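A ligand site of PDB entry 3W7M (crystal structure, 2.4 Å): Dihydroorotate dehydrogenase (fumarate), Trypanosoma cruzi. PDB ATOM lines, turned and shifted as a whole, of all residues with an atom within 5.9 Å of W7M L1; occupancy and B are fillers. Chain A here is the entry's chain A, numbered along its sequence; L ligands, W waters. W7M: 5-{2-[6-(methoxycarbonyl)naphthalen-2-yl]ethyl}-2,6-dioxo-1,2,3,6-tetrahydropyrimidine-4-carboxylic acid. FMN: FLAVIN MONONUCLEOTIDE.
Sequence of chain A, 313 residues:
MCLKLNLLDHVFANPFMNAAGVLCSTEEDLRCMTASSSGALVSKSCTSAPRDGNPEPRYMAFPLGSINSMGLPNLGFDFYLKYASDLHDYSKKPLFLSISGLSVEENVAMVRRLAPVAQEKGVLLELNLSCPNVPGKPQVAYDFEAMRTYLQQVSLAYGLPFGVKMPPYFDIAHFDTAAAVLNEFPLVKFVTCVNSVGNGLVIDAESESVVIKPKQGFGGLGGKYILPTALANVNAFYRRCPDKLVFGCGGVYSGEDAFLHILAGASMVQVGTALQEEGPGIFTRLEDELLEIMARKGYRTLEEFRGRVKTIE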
ATOM      1  N   LYS A  44      13.730 -12.531  11.545  1.00  0.00           N
ATOM      2  CA  LYS A  44      12.541 -12.066  12.281  1.00  0.00           C
ATOM      3  C   LYS A  44      11.282 -12.788  11.828  1.00  0.00           C
ATOM      4  O   LYS A  44      11.096 -13.042  10.636  1.00  0.00           O
ATOM      5  CB  LYS A  44      12.349 -10.568  12.073  1.00  0.00           C
ATOM      6  CG  LYS A  44      11.040  -9.979  12.584  1.00  0.00           C
ATOM      7  CD  LYS A  44      10.841 -10.113  14.091  1.00  0.00           C
ATOM      8  CE  LYS A  44       9.436  -9.743  14.566  1.00  0.00           C
ATOM      9  NZ  LYS A  44       9.331  -9.578  16.062  1.00  0.00           N
ATOM     10  N   SER A  45      10.378 -13.041  12.777  1.00  0.00           N
ATOM     11  CA  SER A  45       9.155 -13.780  12.523  1.00  0.00           C
ATOM     12  C   SER A  45       8.306 -12.927  11.664  1.00  0.00           C
ATOM     13  O   SER A  45       8.006 -11.827  12.053  1.00  0.00           O
ATOM     14  CB  SER A  45       8.399 -14.104  13.808  1.00  0.00           C
ATOM     15  OG  SER A  45       8.880 -15.285  14.382  1.00  0.00           O
ATOM     16  N   ARG A  51       4.405  -5.254   8.612  1.00  0.00           N
ATOM     17  CA  ARG A  51       3.786  -4.668   9.777  1.00  0.00           C
ATOM     18  C   ARG A  51       4.701  -3.644  10.433  1.00  0.00           C
ATOM     19  O   ARG A  51       5.912  -3.864  10.544  1.00  0.00           O
ATOM     20  CB  ARG A  51       3.495  -5.757  10.819  1.00  0.00           C
ATOM     21  CG  ARG A  51       2.478  -6.775  10.389  1.00  0.00           C
ATOM     22  CD  ARG A  51       2.422  -7.891  11.405  1.00  0.00           C
ATOM     23  NE  ARG A  51       2.170  -7.441  12.783  1.00  0.00           N
ATOM     24  CZ  ARG A  51       0.958  -7.282  13.296  1.00  0.00           C
ATOM     25  NH1 ARG A  51      -0.113  -7.529  12.552  1.00  0.00           N
ATOM     26  NH2 ARG A  51       0.820  -6.873  14.541  1.00  0.00           N
ATOM     27  N   ASN A  54       3.648  -2.503  17.260  1.00  0.00           N
ATOM     28  CA  ASN A  54       3.034  -1.672  18.273  1.00  0.00           C
ATOM     29  C   ASN A  54       3.793  -0.337  18.405  1.00  0.00           C
ATOM     30  O   ASN A  54       4.963  -0.265  18.005  1.00  0.00           O
ATOM     31  CB  ASN A  54       3.111  -2.377  19.614  1.00  0.00           C
ATOM     32  CG  ASN A  54       2.193  -3.585  19.719  1.00  0.00           C
ATOM     33  OD1 ASN A  54       1.249  -3.763  18.943  1.00  0.00           O
ATOM     34  ND2 ASN A  54       2.498  -4.434  20.713  1.00  0.00           N
ATOM     35  N   ASN A  68       9.271  -6.749  26.308  1.00  0.00           N
ATOM     36  CA  ASN A  68       8.858  -6.297  24.997  1.00  0.00           C
ATOM     37  C   ASN A  68       7.404  -6.540  24.649  1.00  0.00           C
ATOM     38  O   ASN A  68       6.799  -7.575  24.956  1.00  0.00           O
ATOM     39  CB  ASN A  68       9.784  -6.872  23.919  1.00  0.00           C
ATOM     40  CG  ASN A  68       9.310  -8.223  23.383  1.00  0.00           C
ATOM     41  OD1 ASN A  68       8.365  -8.305  22.563  1.00  0.00           O
ATOM     42  ND2 ASN A  68       9.992  -9.285  23.799  1.00  0.00           N
ATOM     43  N   SER A  69       6.807  -5.580  23.997  1.00  0.00           N
ATOM     44  CA  SER A  69       5.595  -5.895  23.287  1.00  0.00           C
ATOM     45  C   SER A  69       5.720  -5.289  21.922  1.00  0.00           C
ATOM     46  O   SER A  69       5.142  -4.223  21.682  1.00  0.00           O
ATOM     47  CB  SER A  69       4.350  -5.428  24.009  1.00  0.00           C
ATOM     48  OG  SER A  69       3.235  -5.915  23.283  1.00  0.00           O
ATOM     49  N   MET A  70       6.496  -5.957  21.050  1.00  0.00           N
ATOM     50  CA  MET A  70       6.836  -5.390  19.741  1.00  0.00           C
ATOM     51  C   MET A  70       5.599  -5.433  18.779  1.00  0.00           C
ATOM     52  O   MET A  70       5.397  -4.540  17.973  1.00  0.00           O
ATOM     53  CB  MET A  70       8.013  -6.111  19.058  1.00  0.00           C
ATOM     54  CG  MET A  70       9.263  -6.316  19.911  1.00  0.00           C
ATOM     55  SD  MET A  70      10.195  -4.819  20.224  1.00  0.00           S
ATOM     56  CE  MET A  70      10.911  -4.422  18.622  1.00  0.00           C
ATOM     57  N   GLY A  71       4.804  -6.479  18.895  1.00  0.00           N
ATOM     58  CA  GLY A  71       3.651  -6.632  18.034  1.00  0.00           C
ATOM     59  C   GLY A  71       3.961  -7.082  16.626  1.00  0.00           C
ATOM     60  O   GLY A  71       3.294  -6.676  15.686  1.00  0.00           O
ATOM     61  N   LEU A  72       5.026  -7.873  16.494  1.00  0.00           N
ATOM     62  CA  LEU A  72       5.402  -8.507  15.246  1.00  0.00           C
ATOM     63  C   LEU A  72       5.742  -7.550  14.093  1.00  0.00           C
ATOM     64  O   LEU A  72       5.297  -7.727  12.956  1.00  0.00           O
ATOM     65  CB  LEU A  72       4.297  -9.445  14.850  1.00  0.00           C
ATOM     66  CG  LEU A  72       4.559 -10.579  13.923  1.00  0.00           C
ATOM     67  CD1 LEU A  72       5.791 -11.378  14.326  1.00  0.00           C
ATOM     68  CD2 LEU A  72       3.305 -11.451  13.935  1.00  0.00           C
ATOM     69  N   PRO A  73       6.556  -6.533  14.389  1.00  0.00           N
ATOM     70  CA  PRO A  73       7.062  -5.705  13.296  1.00  0.00           C
ATOM     71  C   PRO A  73       7.999  -6.519  12.420  1.00  0.00           C
ATOM     72  O   PRO A  73       8.864  -7.180  12.928  1.00  0.00           O
ATOM     73  CB  PRO A  73       7.882  -4.637  14.022  1.00  0.00           C
ATOM     74  CG  PRO A  73       8.342  -5.328  15.257  1.00  0.00           C
ATOM     75  CD  PRO A  73       7.225  -6.263  15.663  1.00  0.00           C
ATOM     76  N   SER A 100       5.491 -16.512  11.644  1.00  0.00           N
ATOM     77  CA  SER A 100       4.490 -16.362  12.667  1.00  0.00           C
ATOM     78  C   SER A 100       3.196 -15.691  12.229  1.00  0.00           C
ATOM     79  O   SER A 100       2.787 -14.684  12.738  1.00  0.00           O
ATOM     80  CB  SER A 100       5.096 -15.584  13.819  1.00  0.00           C
ATOM     81  OG  SER A 100       4.125 -15.319  14.749  1.00  0.00           O
ATOM     82  N   LEU A 102      -0.853 -15.022  11.526  1.00  0.00           N
ATOM     83  CA  LEU A 102      -1.903 -14.736  12.484  1.00  0.00           C
ATOM     84  C   LEU A 102      -3.106 -15.651  12.377  1.00  0.00           C
ATOM     85  O   LEU A 102      -4.087 -15.475  13.018  1.00  0.00           O
ATOM     86  CB  LEU A 102      -2.267 -13.247  12.518  1.00  0.00           C
ATOM     87  CG  LEU A 102      -1.055 -12.338  12.781  1.00  0.00           C
ATOM     88  CD1 LEU A 102      -1.319 -10.894  12.487  1.00  0.00           C
ATOM     89  CD2 LEU A 102      -0.475 -12.494  14.151  1.00  0.00           C
ATOM     90  N   ASN A 128       6.640 -20.346  14.517  1.00  0.00           N
ATOM     91  CA  ASN A 128       6.449 -19.718  15.819  1.00  0.00           C
ATOM     92  C   ASN A 128       5.049 -19.996  16.350  1.00  0.00           C
ATOM     93  O   ASN A 128       4.058 -19.427  15.876  1.00  0.00           O
ATOM     94  CB  ASN A 128       6.729 -18.202  15.725  1.00  0.00           C
ATOM     95  CG  ASN A 128       6.601 -17.485  17.050  1.00  0.00           C
ATOM     96  OD1 ASN A 128       6.407 -18.081  18.111  1.00  0.00           O
ATOM     97  ND2 ASN A 128       6.737 -16.176  17.006  1.00  0.00           N
ATOM     98  N   SER A 130       4.055 -19.565  19.373  1.00  0.00           N
ATOM     99  CA  SER A 130       3.750 -18.689  20.449  1.00  0.00           C
ATOM    100  C   SER A 130       2.999 -17.501  19.932  1.00  0.00           C
ATOM    101  O   SER A 130       2.906 -16.536  20.588  1.00  0.00           O
ATOM    102  CB  SER A 130       4.994 -18.326  21.233  1.00  0.00           C
ATOM    103  OG  SER A 130       4.777 -17.155  21.934  1.00  0.00           O
ATOM    104  N   CYS A 131       2.507 -17.590  18.724  1.00  0.00           N
ATOM    105  CA  CYS A 131       1.678 -16.596  18.151  1.00  0.00           C
ATOM    106  C   CYS A 131       0.317 -16.454  18.816  1.00  0.00           C
ATOM    107  O   CYS A 131      -0.265 -17.409  19.281  1.00  0.00           O
ATOM    108  CB  CYS A 131       1.474 -16.911  16.686  1.00  0.00           C
ATOM    109  SG  CYS A 131       1.474 -15.418  15.736  1.00  0.00           S
ATOM    110  N   PRO A 132      -0.166 -15.141  18.852  1.00  0.00           N
ATOM    111  CA  PRO A 132      -1.576 -15.045  19.209  1.00  0.00           C
ATOM    112  C   PRO A 132      -2.482 -15.615  18.132  1.00  0.00           C
ATOM    113  O   PRO A 132      -2.183 -15.610  16.984  1.00  0.00           O
ATOM    114  CB  PRO A 132      -1.803 -13.556  19.330  1.00  0.00           C
ATOM    115  CG  PRO A 132      -0.920 -12.992  18.305  1.00  0.00           C
ATOM    116  CD  PRO A 132       0.315 -13.678  18.697  1.00  0.00           C
ATOM    117  N   LYS A 165       8.693 -23.208  17.524  1.00  0.00           N
ATOM    118  CA  LYS A 165       9.182 -22.389  18.645  1.00  0.00           C
ATOM    119  C   LYS A 165       8.106 -22.311  19.726  1.00  0.00           C
ATOM    120  O   LYS A 165       7.028 -21.785  19.468  1.00  0.00           O
ATOM    121  CB  LYS A 165       9.586 -20.992  18.122  1.00  0.00           C
ATOM    122  CG  LYS A 165       9.848 -19.899  19.131  1.00  0.00           C
ATOM    123  CD  LYS A 165      11.251 -19.944  19.702  1.00  0.00           C
ATOM    124  CE  LYS A 165      11.583 -18.706  20.522  1.00  0.00           C
ATOM    125  NZ  LYS A 165      11.871 -17.510  19.674  1.00  0.00           N
ATOM    126  N   ASN A 195      10.231 -19.217  24.165  1.00  0.00           N
ATOM    127  CA  ASN A 195       9.913 -17.841  23.854  1.00  0.00           C
ATOM    128  C   ASN A 195       9.859 -17.059  25.141  1.00  0.00           C
ATOM    129  O   ASN A 195      10.047 -17.620  26.238  1.00  0.00           O
ATOM    130  CB  ASN A 195       8.550 -17.748  23.161  1.00  0.00           C
ATOM    131  CG  ASN A 195       8.485 -16.601  22.178  1.00  0.00           C
ATOM    132  OD1 ASN A 195       8.658 -15.449  22.554  1.00  0.00           O
ATOM    133  ND2 ASN A 195       8.208 -16.903  20.911  1.00  0.00           N
ATOM    134  N   SER A 196       9.541 -15.775  25.044  1.00  0.00           N
ATOM    135  CA  SER A 196       9.493 -14.956  26.220  1.00  0.00           C
ATOM    136  C   SER A 196       8.475 -15.448  27.251  1.00  0.00           C
ATOM    137  O   SER A 196       7.436 -16.007  26.938  1.00  0.00           O
ATOM    138  CB  SER A 196       9.240 -13.504  25.842  1.00  0.00           C
ATOM    139  OG  SER A 196       8.291 -13.360  24.819  1.00  0.00           O
ATOM    140  N   PRO A 214       2.566  -0.229  24.852  1.00  0.00           N
ATOM    141  CA  PRO A 214       1.475  -1.169  24.556  1.00  0.00           C
ATOM    142  C   PRO A 214       0.988  -1.958  25.779  1.00  0.00           C
ATOM    143  O   PRO A 214       1.774  -2.283  26.658  1.00  0.00           O
ATOM    144  CB  PRO A 214       2.113  -2.157  23.548  1.00  0.00           C
ATOM    145  CG  PRO A 214       3.285  -1.463  23.001  1.00  0.00           C
ATOM    146  CD  PRO A 214       3.790  -0.604  24.117  1.00  0.00           C
ATOM    147  N   LYS A 215      -0.309  -2.260  25.794  1.00  0.00           N
ATOM    148  CA  LYS A 215      -0.900  -3.220  26.750  1.00  0.00           C
ATOM    149  C   LYS A 215      -0.727  -2.865  28.206  1.00  0.00           C
ATOM    150  O   LYS A 215      -0.563  -3.731  29.051  1.00  0.00           O
ATOM    151  CB  LYS A 215      -0.301  -4.612  26.525  1.00  0.00           C
ATOM    152  CG  LYS A 215      -0.777  -5.333  25.283  1.00  0.00           C
ATOM    153  CD  LYS A 215      -0.057  -6.662  25.128  1.00  0.00           C
ATOM    154  CE  LYS A 215      -0.319  -7.586  26.313  1.00  0.00           C
ATOM    155  NZ  LYS A 215       0.352  -8.900  26.141  1.00  0.00           N
ATOM    156  N   GLY A 220       6.593  -9.396  27.249  1.00  0.00           N
ATOM    157  CA  GLY A 220       7.280 -10.650  27.319  1.00  0.00           C
ATOM    158  C   GLY A 220       8.630 -10.444  27.966  1.00  0.00           C
ATOM    159  O   GLY A 220       9.306  -9.458  27.633  1.00  0.00           O
HETATM  160  OAB W7M L   1       6.862  -9.286  18.107  1.00  0.00           O
HETATM  161  CAR W7M L   1       6.594  -9.588  19.313  1.00  0.00           C
HETATM  162  OAF W7M L   1       5.969  -8.805  20.079  1.00  0.00           O
HETATM  163  CAV W7M L   1       7.060 -10.776  19.867  1.00  0.00           C
HETATM  164  NAO W7M L   1       7.786 -10.625  21.056  1.00  0.00           N
HETATM  165  CAX W7M L   1       8.280 -11.729  21.712  1.00  0.00           C
HETATM  166  OAD W7M L   1       8.918 -11.590  22.758  1.00  0.00           O
HETATM  167  NAP W7M L   1       8.057 -12.953  21.179  1.00  0.00           N
HETATM  168  CAY W7M L   1       7.338 -13.141  19.994  1.00  0.00           C
HETATM  169  OAE W7M L   1       7.177 -14.302  19.560  1.00  0.00           O
HETATM  170  CAW W7M L   1       6.820 -12.034  19.332  1.00  0.00           C
HETATM  171  CAN W7M L   1       6.077 -12.258  18.172  1.00  0.00           C
HETATM  172  CAM W7M L   1       4.617 -12.736  18.636  1.00  0.00           C
HETATM  173  CAT W7M L   1       3.729 -11.669  18.966  1.00  0.00           C
HETATM  174  CAK W7M L   1       2.841 -11.117  18.029  1.00  0.00           C
HETATM  175  CAG W7M L   1       3.718 -11.162  20.273  1.00  0.00           C
HETATM  176  CAI W7M L   1       2.867 -10.116  20.631  1.00  0.00           C
HETATM  177  CBA W7M L   1       1.985  -9.536  19.708  1.00  0.00           C
HETATM  178  CAL W7M L   1       1.156  -8.479  20.088  1.00  0.00           C
HETATM  179  CAZ W7M L   1       1.955 -10.050  18.389  1.00  0.00           C
HETATM  180  CAJ W7M L   1       1.081  -9.466  17.468  1.00  0.00           C
HETATM  181  CAH W7M L   1       0.254  -8.408  17.879  1.00  0.00           C
HETATM  182  CAU W7M L   1       0.258  -7.884  19.185  1.00  0.00           C
HETATM  183  CAS W7M L   1      -0.650  -6.805  19.520  1.00  0.00           C
HETATM  184  OAC W7M L   1      -1.301  -6.231  18.654  1.00  0.00           O
HETATM  185  OAQ W7M L   1      -0.863  -6.445  20.819  1.00  0.00           O
HETATM  186  CAA W7M L   1       0.247  -6.017  21.587  1.00  0.00           C
HETATM  187  N1  FMN L   2      10.550 -14.739  19.448  1.00  0.00           N
HETATM  188  C2  FMN L   2       9.978 -15.161  18.301  1.00  0.00           C
HETATM  189  O2  FMN L   2       9.725 -16.394  18.187  1.00  0.00           O
HETATM  190  N3  FMN L   2       9.680 -14.332  17.284  1.00  0.00           N
HETATM  191  C4  FMN L   2       9.959 -13.028  17.349  1.00  0.00           C
HETATM  192  O4  FMN L   2       9.733 -12.194  16.425  1.00  0.00           O
HETATM  193  C4A FMN L   2      10.587 -12.513  18.569  1.00  0.00           C
HETATM  194  N5  FMN L   2      10.870 -11.209  18.694  1.00  0.00           N
HETATM  195  C5A FMN L   2      11.476 -10.736  19.799  1.00  0.00           C
HETATM  196  C6  FMN L   2      11.815  -9.384  19.857  1.00  0.00           C
HETATM  197  C7  FMN L   2      12.450  -8.912  20.983  1.00  0.00           C
HETATM  198  C7M FMN L   2      12.761  -7.447  21.052  1.00  0.00           C
HETATM  199  C8  FMN L   2      12.797  -9.806  22.099  1.00  0.00           C
HETATM  200  C8M FMN L   2      13.456  -9.251  23.340  1.00  0.00           C
HETATM  201  C9  FMN L   2      12.467 -11.129  22.040  1.00  0.00           C
HETATM  202  C9A FMN L   2      11.826 -11.644  20.928  1.00  0.00           C
HETATM  203  N10 FMN L   2      11.501 -12.995  20.792  1.00  0.00           N
HETATM  204  C10 FMN L   2      10.871 -13.455  19.632  1.00  0.00           C
HETATM  205  C1' FMN L   2      11.797 -13.930  21.844  1.00  0.00           C
HETATM  206  C2' FMN L   2      13.218 -14.370  21.679  1.00  0.00           C
HETATM  207  O2' FMN L   2      13.304 -15.031  20.426  1.00  0.00           O
HETATM  208  C3' FMN L   2      13.585 -15.286  22.841  1.00  0.00           C
HETATM  209  O3' FMN L   2      12.844 -16.459  22.716  1.00  0.00           O
HETATM  210  C4' FMN L   2      13.323 -14.714  24.234  1.00  0.00           C
HETATM  211  O4' FMN L   2      13.694 -13.337  24.297  1.00  0.00           O
HETATM  212  C5' FMN L   2      14.166 -15.428  25.275  1.00  0.00           C
HETATM  213  O5' FMN L   2      15.550 -15.186  24.918  1.00  0.00           O
HETATM  214  P   FMN L   2      16.516 -14.316  25.873  1.00  0.00           P
HETATM  215  O1P FMN L   2      17.843 -14.679  25.305  1.00  0.00           O
HETATM  216  O2P FMN L   2      16.174 -14.758  27.274  1.00  0.00           O
HETATM  217  O3P FMN L   2      16.062 -12.911  25.642  1.00  0.00           O
HETATM  218  O   HOH W   1       5.651  -9.320  22.685  1.00  0.00           O
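OAD of W7M L1 is in hydrogen-bond range of ND2 of Asn 68. OG of Ser 196 sits at hydrogen-bond distance from OAD of W7M L1. An oxygen (OAB) of W7M L1 sits at hydrogen-bond distance from the backbone NH (N) of Leu 72. The backbone NH (N) of Gly 71 lies within hydrogen-bond range of an oxygen (OAF) of W7M L1, at 2.9 Å. The side-chain amide oxygen (OD1) of Asn 195 sits at hydrogen-bond distance from a nitrogen (NAP) of W7M L1, 2.9 Å away. The backbone NH (N) of Met 70 is in hydrogen-bond range of an oxygen (OAF) of W7M L1 (3.1 Å). ND2 of Asn 128 lies within hydrogen-bond range of OAE of W7M L1, 3.2 Å away. OAB of W7M L1 is in salt-bridge range of NZ of Lys 44 (3.2 Å). The side-chain amide nitrogen (ND2) of Asn 195 lies within hydrogen-bond range of an oxygen (O2) of FMN L2 (3.2 Å). The side-chain amide nitrogen of Asn 128 is in hydrogen-bond range of an oxygen (O2) of FMN L2 (3.2 Å). The side-chain amino group (NZ) of Lys 44 is in hydrogen-bond range of an oxygen (O4) of FMN L2 (2.7 Å). The side-chain hydroxyl (OG) of Ser 45 is in hydrogen-bond range of a nitrogen (N3) of FMN L2. The side-chain amino group (NZ) of Lys 165 sits at hydrogen-bond distance from an oxygen (O2) of FMN L2, at 2.8 Å.
OAE of W7M L1 sits close to N3 of FMN L2, 3.4 Å away.
N of Met 70 is in hydrogen-bond range of OD1 of Asn 68, 3.4 Å away. O of Asn 68 lies within hydrogen-bond range of N of Gly 220, at 2.9 Å. The side-chain amide oxygen (OD1) of Asn 195 lies within hydrogen-bond range of the side-chain hydroxyl (OG) of Ser 196 (3.1 Å). The guanidinium group (NE) of Arg 51 sits at hydrogen-bond distance from the backbone carbonyl oxygen (O) of Leu 72, 3.1 Å away. The backbone carbonyl oxygen (O) of Gly 71 is in hydrogen-bond range of the guanidinium group (NH2) of Arg 51, at 2.7 Å. The backbone NH (N) of Asn 54 is in hydrogen-bond range of the backbone carbonyl oxygen (O) of Met 70, 2.8 Å away. The side-chain amide nitrogen (ND2) of Asn 54 sits at hydrogen-bond distance from the backbone carbonyl oxygen (O) of Ser 69. The side-chain amide oxygen of Asn 128 is in hydrogen-bond range of the backbone NH of Ser 130 (3.1 Å).
Merely in contact with W7M L1: Arg 51 (3.7 Å), Asn 54 (2.9 Å), Ser 69 (3.4 Å), Pro 73 (3.9 Å), Pro 132 (3.7 Å) and Lys 215 (3.6 Å). Hydrophobic or aromatic side chains within 4 Å of W7M L1: Met 70, Leu 72, Pro 73 and Pro 132. Of the 22 residues printed, 14 come within 4 Å of W7M L1.
Water W1 bridges OAF of W7M L1 (2.7 Å) and OD1 of Asn 68 (2.9 Å).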
